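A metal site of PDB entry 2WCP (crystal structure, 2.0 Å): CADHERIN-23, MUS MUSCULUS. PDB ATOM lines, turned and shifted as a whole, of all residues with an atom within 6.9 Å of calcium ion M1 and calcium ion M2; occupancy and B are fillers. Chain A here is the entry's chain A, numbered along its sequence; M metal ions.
OE2 of Glu 74 lies close to OD1 of Asn 106 (3.1 Å).
O of Gly 101 lies within hydrogen-bond range of N of Glu 22 (2.9 Å).
OD1 of Asp 187 is in hydrogen-bond range of N of Asp 189 (3.2 Å).
The backbone NH of Asp 187 lies within hydrogen-bond range of the backbone carbonyl oxygen of Leu 194, 2.9 Å away.
OE2 of Glu 22 is in hydrogen-bond range of N of Arg 73, at 2.9 Å.
The side-chain carboxylate of Asp 102 lies within hydrogen-bond range of the backbone NH of Leu 139.
The backbone NH of Glu 74 lies close to the side-chain carboxylate of Asp 72 (3.2 Å).
O of Arg 192 is in hydrogen-bond range of ND2 of Asn 104, 3.1 Å away.
Of the 26 residues printed, 7 come within 4 Å of calcium ion M1.
The nearest printed residue that does not touch calcium ion M1 is Arg 73 (4.5 Å).
Six residues have an atom within 4 Å of calcium ion M2: Asn 104, Asn 106, Asp 136, Asp 138, Gly 142 and Asp 187.
The nearest printed residue that does not touch calcium ion M2 is Gly 143 (4.4 Å).
Calcium ion M1 is bound by OE1 of Glu 22 (2.3 Å).
OD1 of Asp 102 is bound to calcium ion M1 (2.3 Å).
Calcium ion M1 is bound by the side-chain carboxylate (OD1) of Asp 138, 2.3 Å away.
OE1 of Glu 74 is bound to calcium ion M1.
The side-chain carboxylate (OD1) of Asp 105 binds calcium ion M1 (2.4 Å).
O of Val 103 binds calcium ion M1, at 2.4 Å.
OE2 of Glu 74 binds calcium ion M1 (2.5 Å).
Calcium ion M1 has seven donor atoms within binding distance.
O of Gly 142 is bound to calcium ion M2, 2.3 Å away.
O of Asn 106 is bound to calcium ion M2 (2.3 Å).
OD2 of Asp 136 binds calcium ion M2, at 2.4 Å.
OD1 of Asn 104 binds calcium ion M2.
Calcium ion M2 is bound by OD2 of Asp 138 (2.4 Å).
OD1 of Asp 136 binds calcium ion M2.
The side-chain carboxylate (OD2) of Asp 187 binds calcium ion M2, 2.6 Å away.
Calcium ion M2 has seven donor atoms within binding distance.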
ATOM      1  N   GLU A  22     -28.667  -2.738 -19.879  1.00  0.00           N
ATOM      2  CA  GLU A  22     -28.075  -4.056 -19.740  1.00  0.00           C
ATOM      3  C   GLU A  22     -28.931  -5.004 -18.917  1.00  0.00           C
ATOM      4  O   GLU A  22     -28.712  -6.195 -19.003  1.00  0.00           O
ATOM      5  CB  GLU A  22     -26.656  -4.004 -19.204  1.00  0.00           C
ATOM      6  CG  GLU A  22     -26.530  -3.553 -17.742  1.00  0.00           C
ATOM      7  CD  GLU A  22     -25.112  -3.566 -17.237  1.00  0.00           C
ATOM      8  OE1 GLU A  22     -24.746  -2.681 -16.409  1.00  0.00           O
ATOM      9  OE2 GLU A  22     -24.358  -4.483 -17.635  1.00  0.00           O
ATOM     10  N   ASP A  72     -24.235  -6.953 -21.416  1.00  0.00           N
ATOM     11  CA  ASP A  72     -23.391  -6.734 -20.228  1.00  0.00           C
ATOM     12  C   ASP A  72     -22.497  -5.553 -20.563  1.00  0.00           C
ATOM     13  O   ASP A  72     -21.524  -5.702 -21.282  1.00  0.00           O
ATOM     14  CB  ASP A  72     -22.565  -7.980 -19.910  1.00  0.00           C
ATOM     15  CG  ASP A  72     -21.571  -7.763 -18.743  1.00  0.00           C
ATOM     16  OD1 ASP A  72     -20.680  -8.588 -18.561  1.00  0.00           O
ATOM     17  OD2 ASP A  72     -21.679  -6.735 -18.039  1.00  0.00           O
ATOM     18  N   ARG A  73     -22.842  -4.357 -20.065  1.00  0.00           N
ATOM     19  CA  ARG A  73     -22.119  -3.160 -20.413  1.00  0.00           C
ATOM     20  C   ARG A  73     -20.642  -3.269 -20.063  1.00  0.00           C
ATOM     21  O   ARG A  73     -19.817  -2.678 -20.728  1.00  0.00           O
ATOM     22  CB  ARG A  73     -22.712  -1.918 -19.717  1.00  0.00           C
ATOM     23  CG  ARG A  73     -22.187  -0.563 -20.258  1.00  0.00           C
ATOM     24  CD  ARG A  73     -22.447   0.571 -19.261  1.00  0.00           C
ATOM     25  NE  ARG A  73     -21.635   0.321 -18.087  1.00  0.00           N
ATOM     26  CZ  ARG A  73     -20.356   0.639 -17.978  1.00  0.00           C
ATOM     27  NH1 ARG A  73     -19.672   0.268 -16.907  1.00  0.00           N
ATOM     28  NH2 ARG A  73     -19.739   1.291 -18.956  1.00  0.00           N
ATOM     29  N   GLU A  74     -20.315  -4.026 -19.009  1.00  0.00           N
ATOM     30  CA  GLU A  74     -18.941  -4.187 -18.559  1.00  0.00           C
ATOM     31  C   GLU A  74     -18.146  -5.147 -19.448  1.00  0.00           C
ATOM     32  O   GLU A  74     -16.950  -5.204 -19.342  1.00  0.00           O
ATOM     33  CB  GLU A  74     -18.884  -4.643 -17.083  1.00  0.00           C
ATOM     34  CG  GLU A  74     -19.214  -3.523 -16.056  1.00  0.00           C
ATOM     35  CD  GLU A  74     -20.683  -3.174 -15.924  1.00  0.00           C
ATOM     36  OE1 GLU A  74     -21.027  -1.972 -15.811  1.00  0.00           O
ATOM     37  OE2 GLU A  74     -21.539  -4.065 -15.894  1.00  0.00           O
ATOM     38  N   GLY A 101     -26.915   0.573 -21.667  1.00  0.00           N
ATOM     39  CA  GLY A 101     -27.089   1.369 -20.445  1.00  0.00           C
ATOM     40  C   GLY A 101     -26.669   0.608 -19.207  1.00  0.00           C
ATOM     41  O   GLY A 101     -26.871  -0.606 -19.098  1.00  0.00           O
ATOM     42  N   ASP A 102     -26.050   1.337 -18.270  1.00  0.00           N
ATOM     43  CA  ASP A 102     -25.548   0.719 -17.078  1.00  0.00           C
ATOM     44  C   ASP A 102     -26.607   0.462 -16.039  1.00  0.00           C
ATOM     45  O   ASP A 102     -27.528   1.259 -15.846  1.00  0.00           O
ATOM     46  CB  ASP A 102     -24.477   1.608 -16.457  1.00  0.00           C
ATOM     47  CG  ASP A 102     -23.708   0.910 -15.387  1.00  0.00           C
ATOM     48  OD1 ASP A 102     -23.161  -0.209 -15.630  1.00  0.00           O
ATOM     49  OD2 ASP A 102     -23.638   1.473 -14.285  1.00  0.00           O
ATOM     50  N   VAL A 103     -26.466  -0.674 -15.363  1.00  0.00           N
ATOM     51  CA  VAL A 103     -27.156  -0.914 -14.105  1.00  0.00           C
ATOM     52  C   VAL A 103     -26.059  -1.273 -13.088  1.00  0.00           C
ATOM     53  O   VAL A 103     -24.944  -1.710 -13.458  1.00  0.00           O
ATOM     54  CB  VAL A 103     -28.245  -1.997 -14.282  1.00  0.00           C
ATOM     55  CG1 VAL A 103     -28.498  -2.753 -13.006  1.00  0.00           C
ATOM     56  CG2 VAL A 103     -29.562  -1.376 -14.823  1.00  0.00           C
ATOM     57  N   ASN A 104     -26.348  -1.062 -11.801  1.00  0.00           N
ATOM     58  CA  ASN A 104     -25.396  -1.444 -10.782  1.00  0.00           C
ATOM     59  C   ASN A 104     -25.435  -2.938 -10.550  1.00  0.00           C
ATOM     60  O   ASN A 104     -26.186  -3.397  -9.694  1.00  0.00           O
ATOM     61  CB  ASN A 104     -25.662  -0.733  -9.455  1.00  0.00           C
ATOM     62  CG  ASN A 104     -24.568  -1.014  -8.447  1.00  0.00           C
ATOM     63  OD1 ASN A 104     -23.413  -1.119  -8.868  1.00  0.00           O
ATOM     64  ND2 ASN A 104     -24.895  -1.138  -7.146  1.00  0.00           N
ATOM     65  N   ASP A 105     -24.647  -3.701 -11.298  1.00  0.00           N
ATOM     66  CA  ASP A 105     -24.716  -5.163 -11.228  1.00  0.00           C
ATOM     67  C   ASP A 105     -23.378  -5.805 -10.824  1.00  0.00           C
ATOM     68  O   ASP A 105     -23.238  -7.028 -10.911  1.00  0.00           O
ATOM     69  CB  ASP A 105     -25.309  -5.766 -12.537  1.00  0.00           C
ATOM     70  CG  ASP A 105     -24.542  -5.373 -13.797  1.00  0.00           C
ATOM     71  OD1 ASP A 105     -23.706  -4.418 -13.805  1.00  0.00           O
ATOM     72  OD2 ASP A 105     -24.801  -6.045 -14.836  1.00  0.00           O
ATOM     73  N   ASN A 106     -22.417  -5.007 -10.363  1.00  0.00           N
ATOM     74  CA  ASN A 106     -21.144  -5.528  -9.882  1.00  0.00           C
ATOM     75  C   ASN A 106     -20.859  -5.078  -8.452  1.00  0.00           C
ATOM     76  O   ASN A 106     -21.081  -3.916  -8.126  1.00  0.00           O
ATOM     77  CB  ASN A 106     -20.018  -5.049 -10.777  1.00  0.00           C
ATOM     78  CG  ASN A 106     -20.113  -5.586 -12.170  1.00  0.00           C
ATOM     79  OD1 ASN A 106     -20.794  -4.991 -13.049  1.00  0.00           O
ATOM     80  ND2 ASN A 106     -19.437  -6.681 -12.410  1.00  0.00           N
ATOM     81  N   ALA A 107     -20.377  -5.993  -7.620  1.00  0.00           N
ATOM     82  CA  ALA A 107     -19.785  -5.628  -6.315  1.00  0.00           C
ATOM     83  C   ALA A 107     -18.334  -5.260  -6.530  1.00  0.00           C
ATOM     84  O   ALA A 107     -17.741  -5.633  -7.542  1.00  0.00           O
ATOM     85  CB  ALA A 107     -19.871  -6.793  -5.303  1.00  0.00           C
ATOM     86  N   PRO A 108     -17.728  -4.527  -5.575  1.00  0.00           N
ATOM     87  CA  PRO A 108     -16.333  -4.202  -5.742  1.00  0.00           C
ATOM     88  C   PRO A 108     -15.461  -5.455  -5.669  1.00  0.00           C
ATOM     89  O   PRO A 108     -15.859  -6.445  -5.068  1.00  0.00           O
ATOM     90  CB  PRO A 108     -16.044  -3.266  -4.557  1.00  0.00           C
ATOM     91  CG  PRO A 108     -17.393  -2.699  -4.198  1.00  0.00           C
ATOM     92  CD  PRO A 108     -18.346  -3.806  -4.440  1.00  0.00           C
ATOM     93  N   ASP A 136     -14.671  -1.007  -8.885  1.00  0.00           N
ATOM     94  CA  ASP A 136     -16.074  -1.338  -9.179  1.00  0.00           C
ATOM     95  C   ASP A 136     -16.337  -0.768 -10.559  1.00  0.00           C
ATOM     96  O   ASP A 136     -16.213   0.441 -10.756  1.00  0.00           O
ATOM     97  CB  ASP A 136     -16.999  -0.753  -8.099  1.00  0.00           C
ATOM     98  CG  ASP A 136     -18.425  -1.255  -8.216  1.00  0.00           C
ATOM     99  OD1 ASP A 136     -18.921  -1.343  -9.353  1.00  0.00           O
ATOM    100  OD2 ASP A 136     -19.074  -1.529  -7.211  1.00  0.00           O
ATOM    101  N   PRO A 137     -16.596  -1.642 -11.548  1.00  0.00           N
ATOM    102  CA  PRO A 137     -16.658  -1.184 -12.932  1.00  0.00           C
ATOM    103  C   PRO A 137     -18.009  -0.537 -13.318  1.00  0.00           C
ATOM    104  O   PRO A 137     -18.165  -0.055 -14.440  1.00  0.00           O
ATOM    105  CB  PRO A 137     -16.414  -2.474 -13.704  1.00  0.00           C
ATOM    106  CG  PRO A 137     -17.064  -3.499 -12.857  1.00  0.00           C
ATOM    107  CD  PRO A 137     -16.819  -3.087 -11.430  1.00  0.00           C
ATOM    108  N   ASP A 138     -18.967  -0.486 -12.433  1.00  0.00           N
ATOM    109  CA  ASP A 138     -20.244   0.178 -12.769  1.00  0.00           C
ATOM    110  C   ASP A 138     -20.090   1.691 -12.851  1.00  0.00           C
ATOM    111  O   ASP A 138     -19.049   2.221 -12.507  1.00  0.00           O
ATOM    112  CB  ASP A 138     -21.322  -0.188 -11.776  1.00  0.00           C
ATOM    113  CG  ASP A 138     -21.604  -1.670 -11.754  1.00  0.00           C
ATOM    114  OD1 ASP A 138     -21.914  -2.264 -12.824  1.00  0.00           O
ATOM    115  OD2 ASP A 138     -21.545  -2.234 -10.654  1.00  0.00           O
ATOM    116  N   LEU A 139     -21.117   2.374 -13.354  1.00  0.00           N
ATOM    117  CA  LEU A 139     -21.008   3.819 -13.582  1.00  0.00           C
ATOM    118  C   LEU A 139     -21.597   4.580 -12.396  1.00  0.00           C
ATOM    119  O   LEU A 139     -22.369   4.051 -11.617  1.00  0.00           O
ATOM    120  CB  LEU A 139     -21.685   4.234 -14.875  1.00  0.00           C
ATOM    121  CG  LEU A 139     -21.095   3.615 -16.159  1.00  0.00           C
ATOM    122  CD1 LEU A 139     -21.739   4.255 -17.396  1.00  0.00           C
ATOM    123  CD2 LEU A 139     -19.546   3.740 -16.217  1.00  0.00           C
ATOM    124  N   ALA A 141     -22.559   6.428  -9.006  1.00  0.00           N
ATOM    125  CA  ALA A 141     -22.499   6.064  -7.589  1.00  0.00           C
ATOM    126  C   ALA A 141     -22.295   4.563  -7.411  1.00  0.00           C
ATOM    127  O   ALA A 141     -21.609   4.127  -6.491  1.00  0.00           O
ATOM    128  CB  ALA A 141     -23.770   6.501  -6.872  1.00  0.00           C
ATOM    129  N   GLY A 142     -22.874   3.766  -8.315  1.00  0.00           N
ATOM    130  CA  GLY A 142     -22.687   2.310  -8.277  1.00  0.00           C
ATOM    131  C   GLY A 142     -21.267   1.843  -8.557  1.00  0.00           C
ATOM    132  O   GLY A 142     -20.929   0.663  -8.350  1.00  0.00           O
ATOM    133  N   GLY A 143     -20.439   2.740  -9.054  1.00  0.00           N
ATOM    134  CA  GLY A 143     -19.040   2.446  -9.304  1.00  0.00           C
ATOM    135  C   GLY A 143     -18.070   3.144  -8.350  1.00  0.00           C
ATOM    136  O   GLY A 143     -16.853   3.083  -8.558  1.00  0.00           O
ATOM    137  N   SER A 144     -18.593   3.806  -7.313  1.00  0.00           N
ATOM    138  CA  SER A 144     -17.776   4.654  -6.429  1.00  0.00           C
ATOM    139  C   SER A 144     -17.679   3.984  -5.078  1.00  0.00           C
ATOM    140  O   SER A 144     -18.673   3.861  -4.386  1.00  0.00           O
ATOM    141  CB  SER A 144     -18.419   6.039  -6.319  1.00  0.00           C
ATOM    142  OG  SER A 144     -17.792   6.790  -5.314  1.00  0.00           O
ATOM    143  N   ASP A 187     -20.178  -0.075  -2.954  1.00  0.00           N
ATOM    144  CA  ASP A 187     -20.445   0.998  -3.873  1.00  0.00           C
ATOM    145  C   ASP A 187     -21.502   1.859  -3.210  1.00  0.00           C
ATOM    146  O   ASP A 187     -22.063   1.466  -2.206  1.00  0.00           O
ATOM    147  CB  ASP A 187     -20.864   0.516  -5.303  1.00  0.00           C
ATOM    148  CG  ASP A 187     -22.095  -0.349  -5.311  1.00  0.00           C
ATOM    149  OD1 ASP A 187     -23.067   0.012  -4.622  1.00  0.00           O
ATOM    150  OD2 ASP A 187     -22.096  -1.388  -6.019  1.00  0.00           O
ATOM    151  N   GLN A 188     -21.773   3.019  -3.778  1.00  0.00           N
ATOM    152  CA  GLN A 188     -22.728   3.932  -3.216  1.00  0.00           C
ATOM    153  C   GLN A 188     -24.040   4.017  -3.985  1.00  0.00           C
ATOM    154  O   GLN A 188     -24.655   5.079  -4.056  1.00  0.00           O
ATOM    155  CB  GLN A 188     -22.077   5.301  -3.135  1.00  0.00           C
ATOM    156  CG  GLN A 188     -20.932   5.344  -2.112  1.00  0.00           C
ATOM    157  CD  GLN A 188     -20.221   6.645  -2.208  1.00  0.00           C
ATOM    158  OE1 GLN A 188     -19.157   6.739  -2.816  1.00  0.00           O
ATOM    159  NE2 GLN A 188     -20.847   7.691  -1.686  1.00  0.00           N
ATOM    160  N   ASP A 189     -24.481   2.897  -4.569  1.00  0.00           N
ATOM    161  CA  ASP A 189     -25.786   2.909  -5.249  1.00  0.00           C
ATOM    162  C   ASP A 189     -26.879   3.142  -4.204  1.00  0.00           C
ATOM    163  O   ASP A 189     -26.960   2.461  -3.190  1.00  0.00           O
ATOM    164  CB  ASP A 189     -26.058   1.618  -5.998  1.00  0.00           C
ATOM    165  CG  ASP A 189     -27.258   1.721  -6.931  1.00  0.00           C
ATOM    166  OD1 ASP A 189     -27.166   2.400  -7.993  1.00  0.00           O
ATOM    167  OD2 ASP A 189     -28.290   1.098  -6.612  1.00  0.00           O
ATOM    168  N   ARG A 192     -29.723   0.157  -4.494  1.00  0.00           N
ATOM    169  CA  ARG A 192     -29.217  -1.207  -4.238  1.00  0.00           C
ATOM    170  C   ARG A 192     -27.693  -1.326  -4.170  1.00  0.00           C
ATOM    171  O   ARG A 192     -27.068  -1.844  -5.094  1.00  0.00           O
ATOM    172  CB  ARG A 192     -29.774  -2.183  -5.276  1.00  0.00           C
ATOM    173  CG  ARG A 192     -29.559  -3.662  -4.934  1.00  0.00           C
ATOM    174  CD  ARG A 192     -30.427  -4.572  -5.835  1.00  0.00           C
ATOM    175  NE  ARG A 192     -29.923  -5.954  -5.905  1.00  0.00           N
ATOM    176  CZ  ARG A 192     -28.859  -6.343  -6.623  1.00  0.00           C
ATOM    177  NH1 ARG A 192     -28.499  -7.623  -6.612  1.00  0.00           N
ATOM    178  NH2 ARG A 192     -28.148  -5.470  -7.321  1.00  0.00           N
ATOM    179  N   PRO A 193     -27.090  -0.871  -3.066  1.00  0.00           N
ATOM    180  CA  PRO A 193     -25.632  -0.953  -2.965  1.00  0.00           C
ATOM    181  C   PRO A 193     -25.135  -2.394  -2.937  1.00  0.00           C
ATOM    182  O   PRO A 193     -25.807  -3.269  -2.423  1.00  0.00           O
ATOM    183  CB  PRO A 193     -25.318  -0.256  -1.646  1.00  0.00           C
ATOM    184  CG  PRO A 193     -26.574  -0.300  -0.857  1.00  0.00           C
ATOM    185  CD  PRO A 193     -27.720  -0.398  -1.824  1.00  0.00           C
ATOM    186  N   LEU A 194     -23.950  -2.634  -3.497  1.00  0.00           N
ATOM    187  CA  LEU A 194     -23.342  -3.935  -3.471  1.00  0.00           C
ATOM    188  C   LEU A 194     -21.978  -3.773  -2.777  1.00  0.00           C
ATOM    189  O   LEU A 194     -21.331  -2.737  -2.926  1.00  0.00           O
ATOM    190  CB  LEU A 194     -23.147  -4.459  -4.884  1.00  0.00           C
ATOM    191  CG  LEU A 194     -24.464  -4.581  -5.683  1.00  0.00           C
ATOM    192  CD1 LEU A 194     -24.151  -5.064  -7.071  1.00  0.00           C
ATOM    193  CD2 LEU A 194     -25.394  -5.536  -4.972  1.00  0.00           C
HETATM  194 CA    CA M   1     -23.106  -2.383 -14.817  1.00  0.00          CA
HETATM  195 CA    CA M   2     -21.124  -1.589  -8.372  1.00  0.00          CA
